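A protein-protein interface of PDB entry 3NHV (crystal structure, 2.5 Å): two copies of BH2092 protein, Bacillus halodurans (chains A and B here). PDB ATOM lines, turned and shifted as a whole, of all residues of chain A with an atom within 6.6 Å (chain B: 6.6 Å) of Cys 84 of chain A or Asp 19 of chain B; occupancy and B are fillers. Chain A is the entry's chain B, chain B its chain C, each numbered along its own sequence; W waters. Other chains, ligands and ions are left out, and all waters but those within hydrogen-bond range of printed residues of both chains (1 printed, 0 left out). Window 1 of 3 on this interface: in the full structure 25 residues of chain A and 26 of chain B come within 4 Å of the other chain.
N of Gly 86 of chain A lies within hydrogen-bond range of SG of Cys 84 of chain A, at 3.1 Å.
O of Glu 103 of chain B sits at hydrogen-bond distance from N of Thr 18 of chain B (3.1 Å).
The backbone NH (N) of Ala 21 of chain B is in hydrogen-bond range of the side-chain carboxylate (OD1) of Asp 19 of chain B, at 2.8 Å.
O of Ile 20 of chain B sits at hydrogen-bond distance from OG of Ser 24 of chain B (3.2 Å).
O of Thr 18 of chain B sits at hydrogen-bond distance from N of Ile 105 of chain B, at 3.1 Å.
SG of Cys 79 of chain A is disulfide-bonded to SG of Cys 84 of chain A (2.0 Å).
Of the 13 printed residues of chain A, 5 touch a printed residue of chain B.
Hydrophobic or aromatic side chains of chain A that line the printed part of chain B: Ala 83.
Hydrophobic or aromatic side chains of chain B within 4 Å of the printed part of chain A: Ile 20 and Ile 105.
Among the printed residues, 13 pairs touch across the chains.
Among the printed residues, Asp or Glu carboxylates within 4 Å of a Lys or Arg side-chain nitrogen of the other chain: Lys 89 of chain A with Asp 19 of chain B (3.7 Å) and Lys 89 of chain A with Asp 22 of chain B (3.3 Å).
Among the printed residues, pairs that only touch across the chains: Asn 85 of chain A with Ile 105 of chain B, Ala 83 of chain A with Asp 19 of chain B, Ala 83 of chain A with Glu 114 of chain B, Asn 85 of chain A with Glu 17 of chain B, Pro 82 of chain A with Ile 105 of chain B, Cys 84 of chain A with Asp 19 of chain B, Ala 83 of chain A with Ile 20 of chain B, Cys 84 of chain A with Ile 105 of chain B, Asn 85 of chain A with Thr 18 of chain B and Ala 83 of chain A with Gly 106 of chain B.
Position printed for both chains: 103.
Printed residues of chain A within 4 Å of Glu 17 of chain B: Asn 85.
Printed residues of chain A within 4 Å of Thr 18 of chain B: Asn 85 (3.9 Å).
Of chain A, only Ala 83 (3.2 Å), Cys 84 (3.7 Å), Asn 85 (2.8 Å) and Lys 89 (3.7 Å) come within 4 Å of Asp 19 of chain B.
Printed residues of chain A within 4 Å of Asp 22 of chain B: Lys 89 (3.3 Å).
Ser 24 of chain B touches none of the printed residues of chain A.
Leu 104 of chain B touches none of the printed residues of chain A.
Of the printed residues of chain A, Glu 114 of chain B touches Ala 83 (3.3 Å).
The nearest residue of chain B that does not touch Cys 84 of chain A is Glu 114 of chain B (5.5 Å).
The nearest residue of chain A that does not touch Asp 19 of chain B is Gly 86 of chain A (4.3 Å).
The nearest printed residue of chain A that does not touch Gly 106 of chain B is Pro 82 of chain A (5.0 Å).
The side-chain carboxylate (OD2) of Asp 22 of chain B lies within salt-bridge range of the side-chain amino group (NZ) of Lys 89 of chain A, 3.3 Å away.
The side-chain carboxylate (OD2) of Asp 19 of chain B is in hydrogen-bond range of the backbone NH (N) of Asn 85 of chain A (2.8 Å).
NZ of Lys 89 of chain A lies within salt-bridge range of OD2 of Asp 19 of chain B (3.7 Å).
Water W1 lies within hydrogen-bond range of O of Ala 83 of chain A, OE1 of Glu 114 of chain B and N of Ala 21 of chain B.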
ATOM      1  N   ARG A  40      18.848 -29.304  20.331  1.00  0.00           N
ATOM      2  CA  ARG A  40      19.280 -30.647  20.703  1.00  0.00           C
ATOM      3  C   ARG A  40      19.041 -31.652  19.576  1.00  0.00           C
ATOM      4  O   ARG A  40      18.657 -31.289  18.463  1.00  0.00           O
ATOM      5  CB  ARG A  40      18.532 -31.126  21.950  1.00  0.00           C
ATOM      6  CG  ARG A  40      18.528 -30.160  23.118  1.00  0.00           C
ATOM      7  CD  ARG A  40      17.128 -30.102  23.718  1.00  0.00           C
ATOM      8  NE  ARG A  40      16.808 -31.207  24.618  1.00  0.00           N
ATOM      9  CZ  ARG A  40      15.608 -31.779  24.682  1.00  0.00           C
ATOM     10  NH1 ARG A  40      14.630 -31.364  23.887  1.00  0.00           N
ATOM     11  NH2 ARG A  40      15.370 -32.738  25.570  1.00  0.00           N
ATOM     12  N   CYS A  79      19.190 -25.541  24.757  1.00  0.00           N
ATOM     13  CA  CYS A  79      19.739 -26.889  24.795  1.00  0.00           C
ATOM     14  C   CYS A  79      19.174 -27.554  26.044  1.00  0.00           C
ATOM     15  O   CYS A  79      18.120 -27.159  26.527  1.00  0.00           O
ATOM     16  CB  CYS A  79      21.274 -26.853  24.855  1.00  0.00           C
ATOM     17  SG  CYS A  79      22.035 -28.497  25.141  1.00  0.00           S
ATOM     18  N   TRP A  80      19.863 -28.555  26.575  1.00  0.00           N
ATOM     19  CA  TRP A  80      19.374 -29.234  27.758  1.00  0.00           C
ATOM     20  C   TRP A  80      19.324 -28.345  28.980  1.00  0.00           C
ATOM     21  O   TRP A  80      18.269 -28.194  29.591  1.00  0.00           O
ATOM     22  CB  TRP A  80      20.220 -30.463  28.069  1.00  0.00           C
ATOM     23  CG  TRP A  80      19.993 -31.570  27.109  1.00  0.00           C
ATOM     24  CD1 TRP A  80      20.658 -31.790  25.937  1.00  0.00           C
ATOM     25  CD2 TRP A  80      19.002 -32.596  27.209  1.00  0.00           C
ATOM     26  NE1 TRP A  80      20.141 -32.893  25.300  1.00  0.00           N
ATOM     27  CE2 TRP A  80      19.121 -33.406  26.058  1.00  0.00           C
ATOM     28  CE3 TRP A  80      18.019 -32.907  28.155  1.00  0.00           C
ATOM     29  CZ2 TRP A  80      18.302 -34.512  25.831  1.00  0.00           C
ATOM     30  CZ3 TRP A  80      17.199 -34.011  27.929  1.00  0.00           C
ATOM     31  CH2 TRP A  80      17.347 -34.798  26.772  1.00  0.00           C
ATOM     32  N   GLY A  81      20.463 -27.758  29.335  1.00  0.00           N
ATOM     33  CA  GLY A  81      20.515 -26.895  30.505  1.00  0.00           C
ATOM     34  C   GLY A  81      21.831 -26.155  30.713  1.00  0.00           C
ATOM     35  O   GLY A  81      22.613 -25.987  29.774  1.00  0.00           O
ATOM     36  N   PRO A  82      22.105 -25.712  31.952  1.00  0.00           N
ATOM     37  CA  PRO A  82      23.306 -24.975  32.370  1.00  0.00           C
ATOM     38  C   PRO A  82      24.632 -25.591  31.947  1.00  0.00           C
ATOM     39  O   PRO A  82      25.582 -24.885  31.619  1.00  0.00           O
ATOM     40  CB  PRO A  82      23.179 -24.942  33.892  1.00  0.00           C
ATOM     41  CG  PRO A  82      21.719 -24.952  34.106  1.00  0.00           C
ATOM     42  CD  PRO A  82      21.237 -25.980  33.112  1.00  0.00           C
ATOM     43  N   ALA A  83      24.688 -26.915  31.972  1.00  0.00           N
ATOM     44  CA  ALA A  83      25.911 -27.626  31.626  1.00  0.00           C
ATOM     45  C   ALA A  83      26.056 -27.905  30.135  1.00  0.00           C
ATOM     46  O   ALA A  83      26.807 -28.794  29.740  1.00  0.00           O
ATOM     47  CB  ALA A  83      25.980 -28.935  32.402  1.00  0.00           C
ATOM     48  N   CYS A  84      25.352 -27.148  29.305  1.00  0.00           N
ATOM     49  CA  CYS A  84      25.428 -27.373  27.875  1.00  0.00           C
ATOM     50  C   CYS A  84      25.894 -26.131  27.117  1.00  0.00           C
ATOM     51  O   CYS A  84      25.656 -25.004  27.549  1.00  0.00           O
ATOM     52  CB  CYS A  84      24.062 -27.851  27.359  1.00  0.00           C
ATOM     53  SG  CYS A  84      23.999 -28.136  25.556  1.00  0.00           S
ATOM     54  N   ASN A  85      26.570 -26.356  25.992  1.00  0.00           N
ATOM     55  CA  ASN A  85      27.097 -25.293  25.132  1.00  0.00           C
ATOM     56  C   ASN A  85      26.315 -25.224  23.826  1.00  0.00           C
ATOM     57  O   ASN A  85      26.532 -24.325  23.009  1.00  0.00           O
ATOM     58  CB  ASN A  85      28.563 -25.570  24.783  1.00  0.00           C
ATOM     59  CG  ASN A  85      29.525 -24.996  25.799  1.00  0.00           C
ATOM     60  OD1 ASN A  85      29.157 -24.775  26.954  1.00  0.00           O
ATOM     61  ND2 ASN A  85      30.768 -24.759  25.379  1.00  0.00           N
ATOM     62  N   GLY A  86      25.425 -26.194  23.631  1.00  0.00           N
ATOM     63  CA  GLY A  86      24.631 -26.256  22.416  1.00  0.00           C
ATOM     64  C   GLY A  86      24.026 -24.947  21.962  1.00  0.00           C
ATOM     65  O   GLY A  86      24.248 -24.506  20.835  1.00  0.00           O
ATOM     66  N   ALA A  87      23.263 -24.321  22.848  1.00  0.00           N
ATOM     67  CA  ALA A  87      22.602 -23.068  22.532  1.00  0.00           C
ATOM     68  C   ALA A  87      23.590 -21.978  22.145  1.00  0.00           C
ATOM     69  O   ALA A  87      23.308 -21.154  21.271  1.00  0.00           O
ATOM     70  CB  ALA A  87      21.754 -22.615  23.722  1.00  0.00           C
ATOM     71  N   THR A  88      24.747 -21.964  22.796  1.00  0.00           N
ATOM     72  CA  THR A  88      25.751 -20.953  22.497  1.00  0.00           C
ATOM     73  C   THR A  88      26.369 -21.211  21.124  1.00  0.00           C
ATOM     74  O   THR A  88      26.539 -20.283  20.337  1.00  0.00           O
ATOM     75  CB  THR A  88      26.842 -20.926  23.575  1.00  0.00           C
ATOM     76  OG1 THR A  88      26.221 -20.975  24.869  1.00  0.00           O
ATOM     77  CG2 THR A  88      27.658 -19.639  23.467  1.00  0.00           C
ATOM     78  N   LYS A  89      26.691 -22.465  20.819  1.00  0.00           N
ATOM     79  CA  LYS A  89      27.263 -22.756  19.508  1.00  0.00           C
ATOM     80  C   LYS A  89      26.211 -22.393  18.456  1.00  0.00           C
ATOM     81  O   LYS A  89      26.527 -21.812  17.407  1.00  0.00           O
ATOM     82  CB  LYS A  89      27.640 -24.237  19.381  1.00  0.00           C
ATOM     83  CG  LYS A  89      28.703 -24.731  20.375  1.00  0.00           C
ATOM     84  CD  LYS A  89      29.122 -26.164  20.041  1.00  0.00           C
ATOM     85  CE  LYS A  89      30.127 -26.752  21.040  1.00  0.00           C
ATOM     86  NZ  LYS A  89      29.538 -27.109  22.374  1.00  0.00           N
ATOM     87  N   GLU A 103      20.283 -16.693  23.462  1.00  0.00           N
ATOM     88  CA  GLU A 103      20.253 -18.063  23.973  1.00  0.00           C
ATOM     89  C   GLU A 103      19.470 -18.088  25.273  1.00  0.00           C
ATOM     90  O   GLU A 103      19.503 -17.126  26.043  1.00  0.00           O
ATOM     91  CB  GLU A 103      21.668 -18.600  24.216  1.00  0.00           C
ATOM     92  CG  GLU A 103      22.442 -17.881  25.314  1.00  0.00           C
ATOM     93  CD  GLU A 103      23.894 -18.330  25.411  1.00  0.00           C
ATOM     94  OE1 GLU A 103      24.139 -19.550  25.566  1.00  0.00           O
ATOM     95  OE2 GLU A 103      24.790 -17.462  25.334  1.00  0.00           O
ATOM     96  N   GLU B  17      35.623 -21.540  27.457  1.00  0.00           N
ATOM     97  CA  GLU B  17      34.966 -22.603  28.204  1.00  0.00           C
ATOM     98  C   GLU B  17      34.677 -23.866  27.403  1.00  0.00           C
ATOM     99  O   GLU B  17      34.967 -23.949  26.211  1.00  0.00           O
ATOM    100  CB  GLU B  17      33.660 -22.079  28.807  1.00  0.00           C
ATOM    101  CG  GLU B  17      32.647 -21.585  27.780  1.00  0.00           C
ATOM    102  CD  GLU B  17      31.345 -21.085  28.410  1.00  0.00           C
ATOM    103  OE1 GLU B  17      31.400 -20.134  29.226  1.00  0.00           O
ATOM    104  OE2 GLU B  17      30.270 -21.644  28.080  1.00  0.00           O
ATOM    105  N   THR B  18      34.093 -24.843  28.088  1.00  0.00           N
ATOM    106  CA  THR B  18      33.736 -26.118  27.496  1.00  0.00           C
ATOM    107  C   THR B  18      32.719 -26.813  28.407  1.00  0.00           C
ATOM    108  O   THR B  18      32.748 -26.637  29.626  1.00  0.00           O
ATOM    109  CB  THR B  18      34.991 -26.997  27.322  1.00  0.00           C
ATOM    110  OG1 THR B  18      34.603 -28.316  26.925  1.00  0.00           O
ATOM    111  CG2 THR B  18      35.781 -27.065  28.614  1.00  0.00           C
ATOM    112  N   ASP B  19      31.820 -27.596  27.817  1.00  0.00           N
ATOM    113  CA  ASP B  19      30.798 -28.283  28.598  1.00  0.00           C
ATOM    114  C   ASP B  19      31.059 -29.762  28.860  1.00  0.00           C
ATOM    115  O   ASP B  19      32.010 -30.348  28.345  1.00  0.00           O
ATOM    116  CB  ASP B  19      29.412 -28.129  27.946  1.00  0.00           C
ATOM    117  CG  ASP B  19      29.308 -28.820  26.593  1.00  0.00           C
ATOM    118  OD1 ASP B  19      29.965 -29.868  26.401  1.00  0.00           O
ATOM    119  OD2 ASP B  19      28.548 -28.322  25.726  1.00  0.00           O
ATOM    120  N   ILE B  20      30.189 -30.352  29.668  1.00  0.00           N
ATOM    121  CA  ILE B  20      30.287 -31.750  30.029  1.00  0.00           C
ATOM    122  C   ILE B  20      30.346 -32.640  28.791  1.00  0.00           C
ATOM    123  O   ILE B  20      31.065 -33.639  28.768  1.00  0.00           O
ATOM    124  CB  ILE B  20      29.085 -32.163  30.903  1.00  0.00           C
ATOM    125  CG1 ILE B  20      29.036 -31.289  32.159  1.00  0.00           C
ATOM    126  CG2 ILE B  20      29.175 -33.630  31.271  1.00  0.00           C
ATOM    127  CD1 ILE B  20      30.319 -31.288  32.966  1.00  0.00           C
ATOM    128  N   ALA B  21      29.594 -32.272  27.759  1.00  0.00           N
ATOM    129  CA  ALA B  21      29.559 -33.050  26.525  1.00  0.00           C
ATOM    130  C   ALA B  21      30.931 -33.154  25.873  1.00  0.00           C
ATOM    131  O   ALA B  21      31.472 -34.245  25.721  1.00  0.00           O
ATOM    132  CB  ALA B  21      28.566 -32.435  25.545  1.00  0.00           C
ATOM    133  N   ASP B  22      31.494 -32.016  25.487  1.00  0.00           N
ATOM    134  CA  ASP B  22      32.798 -32.015  24.847  1.00  0.00           C
ATOM    135  C   ASP B  22      33.862 -32.700  25.713  1.00  0.00           C
ATOM    136  O   ASP B  22      34.777 -33.327  25.190  1.00  0.00           O
ATOM    137  CB  ASP B  22      33.238 -30.582  24.523  1.00  0.00           C
ATOM    138  CG  ASP B  22      32.191 -29.807  23.737  1.00  0.00           C
ATOM    139  OD1 ASP B  22      31.437 -30.431  22.953  1.00  0.00           O
ATOM    140  OD2 ASP B  22      32.130 -28.563  23.891  1.00  0.00           O
ATOM    141  N   LEU B  23      33.741 -32.591  27.032  1.00  0.00           N
ATOM    142  CA  LEU B  23      34.724 -33.201  27.916  1.00  0.00           C
ATOM    143  C   LEU B  23      34.656 -34.716  27.828  1.00  0.00           C
ATOM    144  O   LEU B  23      35.663 -35.383  27.611  1.00  0.00           O
ATOM    145  CB  LEU B  23      34.482 -32.785  29.371  1.00  0.00           C
ATOM    146  CG  LEU B  23      35.709 -32.556  30.269  1.00  0.00           C
ATOM    147  CD1 LEU B  23      35.275 -32.601  31.722  1.00  0.00           C
ATOM    148  CD2 LEU B  23      36.781 -33.599  30.011  1.00  0.00           C
ATOM    149  N   SER B  24      33.457 -35.252  28.021  1.00  0.00           N
ATOM    150  CA  SER B  24      33.244 -36.689  27.986  1.00  0.00           C
ATOM    151  C   SER B  24      33.819 -37.318  26.721  1.00  0.00           C
ATOM    152  O   SER B  24      34.288 -38.458  26.744  1.00  0.00           O
ATOM    153  CB  SER B  24      31.754 -36.987  28.080  1.00  0.00           C
ATOM    154  OG  SER B  24      31.061 -36.342  27.032  1.00  0.00           O
ATOM    155  N   GLU B 103      37.557 -23.127  31.245  1.00  0.00           N
ATOM    156  CA  GLU B 103      36.830 -23.541  32.444  1.00  0.00           C
ATOM    157  C   GLU B 103      35.687 -24.477  32.040  1.00  0.00           C
ATOM    158  O   GLU B 103      35.083 -24.312  30.978  1.00  0.00           O
ATOM    159  CB  GLU B 103      36.298 -22.315  33.220  1.00  0.00           C
ATOM    160  CG  GLU B 103      35.353 -21.387  32.448  1.00  0.00           C
ATOM    161  CD  GLU B 103      34.952 -20.124  33.234  1.00  0.00           C
ATOM    162  OE1 GLU B 103      34.529 -20.249  34.407  1.00  0.00           O
ATOM    163  OE2 GLU B 103      35.044 -19.004  32.669  1.00  0.00           O
ATOM    164  N   LEU B 104      35.411 -25.478  32.870  1.00  0.00           N
ATOM    165  CA  LEU B 104      34.347 -26.438  32.586  1.00  0.00           C
ATOM    166  C   LEU B 104      33.058 -26.017  33.257  1.00  0.00           C
ATOM    167  O   LEU B 104      32.952 -26.029  34.481  1.00  0.00           O
ATOM    168  CB  LEU B 104      34.730 -27.827  33.093  1.00  0.00           C
ATOM    169  CG  LEU B 104      33.650 -28.909  33.041  1.00  0.00           C
ATOM    170  CD1 LEU B 104      33.412 -29.377  31.606  1.00  0.00           C
ATOM    171  CD2 LEU B 104      34.098 -30.079  33.900  1.00  0.00           C
ATOM    172  N   ILE B 105      32.070 -25.647  32.461  1.00  0.00           N
ATOM    173  CA  ILE B 105      30.806 -25.242  33.034  1.00  0.00           C
ATOM    174  C   ILE B 105      30.055 -26.492  33.444  1.00  0.00           C
ATOM    175  O   ILE B 105      30.107 -27.514  32.762  1.00  0.00           O
ATOM    176  CB  ILE B 105      29.972 -24.452  32.033  1.00  0.00           C
ATOM    177  CG1 ILE B 105      29.698 -25.325  30.807  1.00  0.00           C
ATOM    178  CG2 ILE B 105      30.710 -23.166  31.672  1.00  0.00           C
ATOM    179  CD1 ILE B 105      28.670 -24.761  29.855  1.00  0.00           C
ATOM    180  N   GLY B 106      29.365 -26.411  34.571  1.00  0.00           N
ATOM    181  CA  GLY B 106      28.629 -27.559  35.045  1.00  0.00           C
ATOM    182  C   GLY B 106      29.347 -28.216  36.202  1.00  0.00           C
ATOM    183  O   GLY B 106      28.705 -28.803  37.072  1.00  0.00           O
ATOM    184  N   GLU B 114      24.821 -36.172  34.539  1.00  0.00           N
ATOM    185  CA  GLU B 114      24.815 -36.607  33.157  1.00  0.00           C
ATOM    186  C   GLU B 114      25.397 -38.011  33.005  1.00  0.00           C
ATOM    187  O   GLU B 114      26.101 -38.314  32.042  1.00  0.00           O
ATOM    188  CB  GLU B 114      25.556 -35.583  32.291  1.00  0.00           C
ATOM    189  CG  GLU B 114      24.669 -34.387  31.971  1.00  0.00           C
ATOM    190  CD  GLU B 114      25.381 -33.261  31.259  1.00  0.00           C
ATOM    191  OE1 GLU B 114      26.111 -33.524  30.285  1.00  0.00           O
ATOM    192  OE2 GLU B 114      25.190 -32.099  31.668  1.00  0.00           O
HETATM  193  O   HOH W   1      26.723 -31.144  28.502  1.00  0.00           O
